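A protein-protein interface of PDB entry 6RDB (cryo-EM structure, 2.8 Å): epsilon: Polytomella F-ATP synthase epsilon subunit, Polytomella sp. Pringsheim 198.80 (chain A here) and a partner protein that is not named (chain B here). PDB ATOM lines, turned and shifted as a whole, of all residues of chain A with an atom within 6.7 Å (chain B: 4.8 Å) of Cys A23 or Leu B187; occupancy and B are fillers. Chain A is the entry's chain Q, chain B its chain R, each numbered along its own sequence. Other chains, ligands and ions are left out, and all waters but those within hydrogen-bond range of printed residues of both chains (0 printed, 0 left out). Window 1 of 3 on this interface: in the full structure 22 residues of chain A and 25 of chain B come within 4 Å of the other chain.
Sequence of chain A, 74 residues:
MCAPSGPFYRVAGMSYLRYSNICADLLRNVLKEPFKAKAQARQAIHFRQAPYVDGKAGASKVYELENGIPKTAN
The backbone carbonyl oxygen (O) of Leu A26 sits at hydrogen-bond distance from the side-chain hydroxyl (OH) of Tyr B188 (2.9 Å).
The side-chain sulfur (SG) of Cys A23 sits close to the backbone carbonyl oxygen (O) of Tyr A19, at 3.7 Å.
NH1 of Arg A28 sits close to O of Ala A24, 3.3 Å away.
Ala B183 touches Tyr A19 (CB to CE2, 3.7 Å).
Tyr A19 touches Glu B186.
O of Cys A23 touches CB of Ser B130 (3.3 Å).
Cys A23 touches Ala B183 (SG to CB, 3.7 Å).
Cys A23 touches Leu B187 (O to CD2, 3.6 Å).
N of Ala A24 touches CB of Ser B130 (3.9 Å).
Ala B184 touches Leu A26.
CD2 of Leu B187 touches CB of Leu A26, at 3.6 Å.
CD1 of Leu A27 touches CD2 of Phe B128, at 3.6 Å.
CG2 of Val A30 touches CE1 of Tyr B188, at 3.7 Å.
Cys A23 touches just these residues of chain B: Ser B130 (3.3 Å), Ala B183 (3.7 Å) and Leu B187 (3.6 Å).
Leu B187 touches just these residues of chain A: Cys A23 (3.6 Å) and Leu A26 (3.6 Å).
Of the printed residues of chain A, Leu B191 touches Val A30.
Of the printed residues of chain B, Leu A27 touches Phe B128 (3.6 Å).
Arg A28 touches none of the printed residues of chain B.
Ala B190 touches none of the printed residues of chain A.
The nearest residue of chain B that does not touch Cys A23 is Pro B113 (4.6 Å).
The nearest printed residue of chain B that does not touch Ala A24 is Leu B187 (5.5 Å).
Printed residues of chain B that touch a printed residue of chain A: Phe B128, Ser B130, Ala B183, Ala B184, Glu B186, Leu B187, Tyr B188 and Leu B191.
Of the 13 printed residues of chain A, 6 touch a printed residue of chain B.
Printed residues of chain A that touch a printed residue of chain B: Tyr A19, Cys A23, Ala A24, Leu A26, Leu A27 and Val A30.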
ATOM      1  N   PHE A   8      24.665   4.610   3.682  1.00  0.00           N
ATOM      2  CA  PHE A   8      25.320   4.278   2.424  1.00  0.00           C
ATOM      3  C   PHE A   8      24.418   4.495   1.221  1.00  0.00           C
ATOM      4  O   PHE A   8      24.923   4.780   0.131  1.00  0.00           O
ATOM      5  CB  PHE A   8      25.835   2.836   2.451  1.00  0.00           C
ATOM      6  CG  PHE A   8      24.758   1.785   2.459  1.00  0.00           C
ATOM      7  CD1 PHE A   8      24.383   1.147   1.287  1.00  0.00           C
ATOM      8  CD2 PHE A   8      24.164   1.393   3.647  1.00  0.00           C
ATOM      9  CE1 PHE A   8      23.411   0.174   1.296  1.00  0.00           C
ATOM     10  CE2 PHE A   8      23.196   0.416   3.664  1.00  0.00           C
ATOM     11  CZ  PHE A   8      22.820  -0.194   2.487  1.00  0.00           C
ATOM     12  N   ARG A  18      13.538   4.362  -2.337  1.00  0.00           N
ATOM     13  CA  ARG A  18      14.048   3.457  -3.358  1.00  0.00           C
ATOM     14  C   ARG A  18      14.929   2.384  -2.746  1.00  0.00           C
ATOM     15  O   ARG A  18      14.957   1.255  -3.242  1.00  0.00           O
ATOM     16  CB  ARG A  18      14.823   4.229  -4.424  1.00  0.00           C
ATOM     17  CG  ARG A  18      15.087   3.422  -5.684  1.00  0.00           C
ATOM     18  CD  ARG A  18      15.868   4.220  -6.692  1.00  0.00           C
ATOM     19  NE  ARG A  18      15.154   5.423  -7.089  1.00  0.00           N
ATOM     20  CZ  ARG A  18      14.299   5.486  -8.101  1.00  0.00           C
ATOM     21  NH1 ARG A  18      14.045   4.407  -8.830  1.00  0.00           N
ATOM     22  NH2 ARG A  18      13.696   6.632  -8.377  1.00  0.00           N
ATOM     23  N   TYR A  19      15.636   2.716  -1.665  1.00  0.00           N
ATOM     24  CA  TYR A  19      16.497   1.744  -1.004  1.00  0.00           C
ATOM     25  C   TYR A  19      15.682   0.636  -0.356  1.00  0.00           C
ATOM     26  O   TYR A  19      15.975  -0.550  -0.536  1.00  0.00           O
ATOM     27  CB  TYR A  19      17.366   2.439   0.044  1.00  0.00           C
ATOM     28  CG  TYR A  19      17.907   1.490   1.084  1.00  0.00           C
ATOM     29  CD1 TYR A  19      17.426   1.507   2.388  1.00  0.00           C
ATOM     30  CD2 TYR A  19      18.891   0.571   0.759  1.00  0.00           C
ATOM     31  CE1 TYR A  19      17.908   0.634   3.331  1.00  0.00           C
ATOM     32  CE2 TYR A  19      19.379  -0.303   1.695  1.00  0.00           C
ATOM     33  CZ  TYR A  19      18.887  -0.268   2.979  1.00  0.00           C
ATOM     34  OH  TYR A  19      19.381  -1.143   3.917  1.00  0.00           O
ATOM     35  N   SER A  20      14.665   1.007   0.415  1.00  0.00           N
ATOM     36  CA  SER A  20      13.887   0.013   1.133  1.00  0.00           C
ATOM     37  C   SER A  20      12.968  -0.773   0.217  1.00  0.00           C
ATOM     38  O   SER A  20      12.568  -1.884   0.574  1.00  0.00           O
ATOM     39  CB  SER A  20      13.074   0.679   2.236  1.00  0.00           C
ATOM     40  OG  SER A  20      12.118  -0.222   2.750  1.00  0.00           O
ATOM     41  N   ASN A  21      12.635  -0.230  -0.952  1.00  0.00           N
ATOM     42  CA  ASN A  21      11.907  -1.009  -1.944  1.00  0.00           C
ATOM     43  C   ASN A  21      12.823  -1.964  -2.691  1.00  0.00           C
ATOM     44  O   ASN A  21      12.372  -3.033  -3.110  1.00  0.00           O
ATOM     45  CB  ASN A  21      11.196  -0.085  -2.929  1.00  0.00           C
ATOM     46  CG  ASN A  21       9.776   0.207  -2.521  1.00  0.00           C
ATOM     47  OD1 ASN A  21       8.898  -0.638  -2.654  1.00  0.00           O
ATOM     48  ND2 ASN A  21       9.541   1.407  -2.014  1.00  0.00           N
ATOM     49  N   ILE A  22      14.092  -1.587  -2.876  1.00  0.00           N
ATOM     50  CA  ILE A  22      15.090  -2.501  -3.431  1.00  0.00           C
ATOM     51  C   ILE A  22      15.264  -3.710  -2.523  1.00  0.00           C
ATOM     52  O   ILE A  22      15.252  -4.855  -2.985  1.00  0.00           O
ATOM     53  CB  ILE A  22      16.419  -1.756  -3.671  1.00  0.00           C
ATOM     54  CG1 ILE A  22      16.388  -1.046  -5.021  1.00  0.00           C
ATOM     55  CG2 ILE A  22      17.613  -2.689  -3.622  1.00  0.00           C
ATOM     56  CD1 ILE A  22      17.492  -0.049  -5.204  1.00  0.00           C
ATOM     57  N   CYS A  23      15.368  -3.479  -1.211  1.00  0.00           N
ATOM     58  CA  CYS A  23      15.443  -4.589  -0.270  1.00  0.00           C
ATOM     59  C   CYS A  23      14.119  -5.335  -0.170  1.00  0.00           C
ATOM     60  O   CYS A  23      14.095  -6.494   0.254  1.00  0.00           O
ATOM     61  CB  CYS A  23      15.878  -4.087   1.103  1.00  0.00           C
ATOM     62  SG  CYS A  23      17.568  -3.477   1.156  1.00  0.00           S
ATOM     63  N   ALA A  24      13.016  -4.696  -0.556  1.00  0.00           N
ATOM     64  CA  ALA A  24      11.752  -5.407  -0.676  1.00  0.00           C
ATOM     65  C   ALA A  24      11.643  -6.140  -2.004  1.00  0.00           C
ATOM     66  O   ALA A  24      11.043  -7.218  -2.059  1.00  0.00           O
ATOM     67  CB  ALA A  24      10.588  -4.433  -0.515  1.00  0.00           C
ATOM     68  N   ASP A  25      12.213  -5.572  -3.073  1.00  0.00           N
ATOM     69  CA  ASP A  25      12.222  -6.234  -4.373  1.00  0.00           C
ATOM     70  C   ASP A  25      13.059  -7.501  -4.338  1.00  0.00           C
ATOM     71  O   ASP A  25      12.659  -8.536  -4.883  1.00  0.00           O
ATOM     72  CB  ASP A  25      12.772  -5.289  -5.441  1.00  0.00           C
ATOM     73  CG  ASP A  25      11.724  -4.356  -5.999  1.00  0.00           C
ATOM     74  OD1 ASP A  25      10.539  -4.482  -5.620  1.00  0.00           O
ATOM     75  OD2 ASP A  25      12.093  -3.479  -6.805  1.00  0.00           O
ATOM     76  N   LEU A  26      14.220  -7.438  -3.690  1.00  0.00           N
ATOM     77  CA  LEU A  26      15.138  -8.567  -3.684  1.00  0.00           C
ATOM     78  C   LEU A  26      14.715  -9.658  -2.717  1.00  0.00           C
ATOM     79  O   LEU A  26      15.167 -10.797  -2.861  1.00  0.00           O
ATOM     80  CB  LEU A  26      16.546  -8.083  -3.357  1.00  0.00           C
ATOM     81  CG  LEU A  26      17.202  -7.109  -4.334  1.00  0.00           C
ATOM     82  CD1 LEU A  26      18.678  -7.065  -4.082  1.00  0.00           C
ATOM     83  CD2 LEU A  26      16.929  -7.513  -5.771  1.00  0.00           C
ATOM     84  N   LEU A  27      13.874  -9.343  -1.735  1.00  0.00           N
ATOM     85  CA  LEU A  27      13.320 -10.405  -0.908  1.00  0.00           C
ATOM     86  C   LEU A  27      12.291 -11.219  -1.681  1.00  0.00           C
ATOM     87  O   LEU A  27      12.240 -12.441  -1.538  1.00  0.00           O
ATOM     88  CB  LEU A  27      12.704  -9.824   0.365  1.00  0.00           C
ATOM     89  CG  LEU A  27      12.059 -10.805   1.350  1.00  0.00           C
ATOM     90  CD1 LEU A  27      12.992 -11.955   1.676  1.00  0.00           C
ATOM     91  CD2 LEU A  27      11.652 -10.104   2.623  1.00  0.00           C
ATOM     92  N   ARG A  28      11.492 -10.567  -2.529  1.00  0.00           N
ATOM     93  CA  ARG A  28      10.465 -11.269  -3.291  1.00  0.00           C
ATOM     94  C   ARG A  28      11.046 -12.201  -4.344  1.00  0.00           C
ATOM     95  O   ARG A  28      10.399 -13.191  -4.696  1.00  0.00           O
ATOM     96  CB  ARG A  28       9.522 -10.273  -3.963  1.00  0.00           C
ATOM     97  CG  ARG A  28       8.763  -9.373  -3.008  1.00  0.00           C
ATOM     98  CD  ARG A  28       7.853  -8.427  -3.766  1.00  0.00           C
ATOM     99  NE  ARG A  28       7.457  -7.285  -2.952  1.00  0.00           N
ATOM    100  CZ  ARG A  28       7.929  -6.056  -3.117  1.00  0.00           C
ATOM    101  NH1 ARG A  28       8.815  -5.811  -4.071  1.00  0.00           N
ATOM    102  NH2 ARG A  28       7.522  -5.075  -2.327  1.00  0.00           N
ATOM    103  N   VAL A  30      13.452 -14.221  -3.920  1.00  0.00           N
ATOM    104  CA  VAL A  30      13.836 -15.466  -3.274  1.00  0.00           C
ATOM    105  C   VAL A  30      12.705 -16.021  -2.403  1.00  0.00           C
ATOM    106  O   VAL A  30      12.964 -16.698  -1.411  1.00  0.00           O
ATOM    107  CB  VAL A  30      15.144 -15.301  -2.480  1.00  0.00           C
ATOM    108  CG1 VAL A  30      16.302 -15.050  -3.427  1.00  0.00           C
ATOM    109  CG2 VAL A  30      15.043 -14.154  -1.510  1.00  0.00           C
ATOM    110  N   PRO B 113      17.772  -5.795   7.268  1.00  0.00           N
ATOM    111  CA  PRO B 113      17.162  -7.068   6.880  1.00  0.00           C
ATOM    112  C   PRO B 113      17.451  -8.158   7.897  1.00  0.00           C
ATOM    113  O   PRO B 113      18.602  -8.559   8.086  1.00  0.00           O
ATOM    114  CB  PRO B 113      17.821  -7.369   5.534  1.00  0.00           C
ATOM    115  CG  PRO B 113      18.104  -6.040   4.970  1.00  0.00           C
ATOM    116  CD  PRO B 113      18.404  -5.124   6.117  1.00  0.00           C
ATOM    117  N   PHE B 128      10.923 -12.831   8.447  1.00  0.00           N
ATOM    118  CA  PHE B 128      12.114 -12.177   7.930  1.00  0.00           C
ATOM    119  C   PHE B 128      11.695 -10.936   7.157  1.00  0.00           C
ATOM    120  O   PHE B 128      10.938 -11.031   6.187  1.00  0.00           O
ATOM    121  CB  PHE B 128      12.911 -13.117   7.031  1.00  0.00           C
ATOM    122  CG  PHE B 128      14.131 -12.487   6.437  1.00  0.00           C
ATOM    123  CD1 PHE B 128      15.268 -12.298   7.200  1.00  0.00           C
ATOM    124  CD2 PHE B 128      14.140 -12.080   5.116  1.00  0.00           C
ATOM    125  CE1 PHE B 128      16.389 -11.717   6.655  1.00  0.00           C
ATOM    126  CE2 PHE B 128      15.258 -11.500   4.567  1.00  0.00           C
ATOM    127  CZ  PHE B 128      16.384 -11.316   5.338  1.00  0.00           C
ATOM    128  N   SER B 130      12.551  -6.926   5.380  1.00  0.00           N
ATOM    129  CA  SER B 130      13.481  -6.338   4.431  1.00  0.00           C
ATOM    130  C   SER B 130      14.209  -5.121   4.976  1.00  0.00           C
ATOM    131  O   SER B 130      15.081  -4.582   4.289  1.00  0.00           O
ATOM    132  CB  SER B 130      12.738  -5.934   3.160  1.00  0.00           C
ATOM    133  OG  SER B 130      11.864  -4.851   3.419  1.00  0.00           O
ATOM    134  N   ALA B 183      23.276  -3.431  -0.568  1.00  0.00           N
ATOM    135  CA  ALA B 183      22.001  -3.888  -0.032  1.00  0.00           C
ATOM    136  C   ALA B 183      21.650  -5.283  -0.530  1.00  0.00           C
ATOM    137  O   ALA B 183      20.924  -6.015   0.148  1.00  0.00           O
ATOM    138  CB  ALA B 183      20.898  -2.901  -0.395  1.00  0.00           C
ATOM    139  N   ALA B 184      22.156  -5.668  -1.703  1.00  0.00           N
ATOM    140  CA  ALA B 184      21.963  -7.032  -2.178  1.00  0.00           C
ATOM    141  C   ALA B 184      22.770  -8.027  -1.355  1.00  0.00           C
ATOM    142  O   ALA B 184      22.330  -9.162  -1.139  1.00  0.00           O
ATOM    143  CB  ALA B 184      22.346  -7.136  -3.652  1.00  0.00           C
ATOM    144  N   ILE B 185      23.952  -7.623  -0.890  1.00  0.00           N
ATOM    145  CA  ILE B 185      24.822  -8.548  -0.172  1.00  0.00           C
ATOM    146  C   ILE B 185      24.301  -8.796   1.238  1.00  0.00           C
ATOM    147  O   ILE B 185      24.089  -9.945   1.637  1.00  0.00           O
ATOM    148  CB  ILE B 185      26.273  -8.031  -0.164  1.00  0.00           C
ATOM    149  CG1 ILE B 185      26.898  -8.179  -1.551  1.00  0.00           C
ATOM    150  CG2 ILE B 185      27.110  -8.775   0.864  1.00  0.00           C
ATOM    151  CD1 ILE B 185      28.012  -7.194  -1.834  1.00  0.00           C
ATOM    152  N   GLU B 186      24.063  -7.723   2.003  1.00  0.00           N
ATOM    153  CA  GLU B 186      23.724  -7.869   3.417  1.00  0.00           C
ATOM    154  C   GLU B 186      22.328  -8.433   3.635  1.00  0.00           C
ATOM    155  O   GLU B 186      22.030  -8.909   4.734  1.00  0.00           O
ATOM    156  CB  GLU B 186      23.841  -6.526   4.135  1.00  0.00           C
ATOM    157  CG  GLU B 186      22.961  -5.432   3.549  1.00  0.00           C
ATOM    158  CD  GLU B 186      22.845  -4.221   4.458  1.00  0.00           C
ATOM    159  OE1 GLU B 186      21.709  -3.865   4.838  1.00  0.00           O
ATOM    160  OE2 GLU B 186      23.890  -3.627   4.795  1.00  0.00           O
ATOM    161  N   LEU B 187      21.470  -8.390   2.619  1.00  0.00           N
ATOM    162  CA  LEU B 187      20.142  -8.975   2.733  1.00  0.00           C
ATOM    163  C   LEU B 187      20.206 -10.494   2.653  1.00  0.00           C
ATOM    164  O   LEU B 187      19.660 -11.192   3.515  1.00  0.00           O
ATOM    165  CB  LEU B 187      19.239  -8.400   1.642  1.00  0.00           C
ATOM    166  CG  LEU B 187      17.909  -9.033   1.251  1.00  0.00           C
ATOM    167  CD1 LEU B 187      16.971  -9.177   2.417  1.00  0.00           C
ATOM    168  CD2 LEU B 187      17.283  -8.153   0.211  1.00  0.00           C
ATOM    169  N   TYR B 188      20.876 -11.023   1.628  1.00  0.00           N
ATOM    170  CA  TYR B 188      20.996 -12.469   1.498  1.00  0.00           C
ATOM    171  C   TYR B 188      21.973 -13.049   2.511  1.00  0.00           C
ATOM    172  O   TYR B 188      21.894 -14.238   2.829  1.00  0.00           O
ATOM    173  CB  TYR B 188      21.429 -12.837   0.082  1.00  0.00           C
ATOM    174  CG  TYR B 188      20.456 -12.421  -0.988  1.00  0.00           C
ATOM    175  CD1 TYR B 188      19.087 -12.580  -0.810  1.00  0.00           C
ATOM    176  CD2 TYR B 188      20.905 -11.866  -2.180  1.00  0.00           C
ATOM    177  CE1 TYR B 188      18.192 -12.197  -1.792  1.00  0.00           C
ATOM    178  CE2 TYR B 188      20.020 -11.478  -3.166  1.00  0.00           C
ATOM    179  CZ  TYR B 188      18.667 -11.649  -2.967  1.00  0.00           C
ATOM    180  OH  TYR B 188      17.784 -11.265  -3.949  1.00  0.00           O
ATOM    181  N   SER B 189      22.902 -12.234   3.020  1.00  0.00           N
ATOM    182  CA  SER B 189      23.825 -12.717   4.040  1.00  0.00           C
ATOM    183  C   SER B 189      23.112 -12.958   5.362  1.00  0.00           C
ATOM    184  O   SER B 189      23.398 -13.936   6.058  1.00  0.00           O
ATOM    185  CB  SER B 189      24.964 -11.724   4.227  1.00  0.00           C
ATOM    186  OG  SER B 189      25.441 -11.272   2.973  1.00  0.00           O
ATOM    187  N   ALA B 190      22.186 -12.073   5.728  1.00  0.00           N
ATOM    188  CA  ALA B 190      21.385 -12.293   6.923  1.00  0.00           C
ATOM    189  C   ALA B 190      20.270 -13.302   6.698  1.00  0.00           C
ATOM    190  O   ALA B 190      19.842 -13.955   7.655  1.00  0.00           O
ATOM    191  CB  ALA B 190      20.797 -10.971   7.412  1.00  0.00           C
ATOM    192  N   LEU B 191      19.796 -13.444   5.459  1.00  0.00           N
ATOM    193  CA  LEU B 191      18.759 -14.420   5.155  1.00  0.00           C
ATOM    194  C   LEU B 191      19.290 -15.846   5.199  1.00  0.00           C
ATOM    195  O   LEU B 191      18.607 -16.738   5.716  1.00  0.00           O
ATOM    196  CB  LEU B 191      18.151 -14.123   3.782  1.00  0.00           C
ATOM    197  CG  LEU B 191      16.977 -14.965   3.282  1.00  0.00           C
ATOM    198  CD1 LEU B 191      15.911 -15.137   4.353  1.00  0.00           C
ATOM    199  CD2 LEU B 191      16.397 -14.333   2.035  1.00  0.00           C
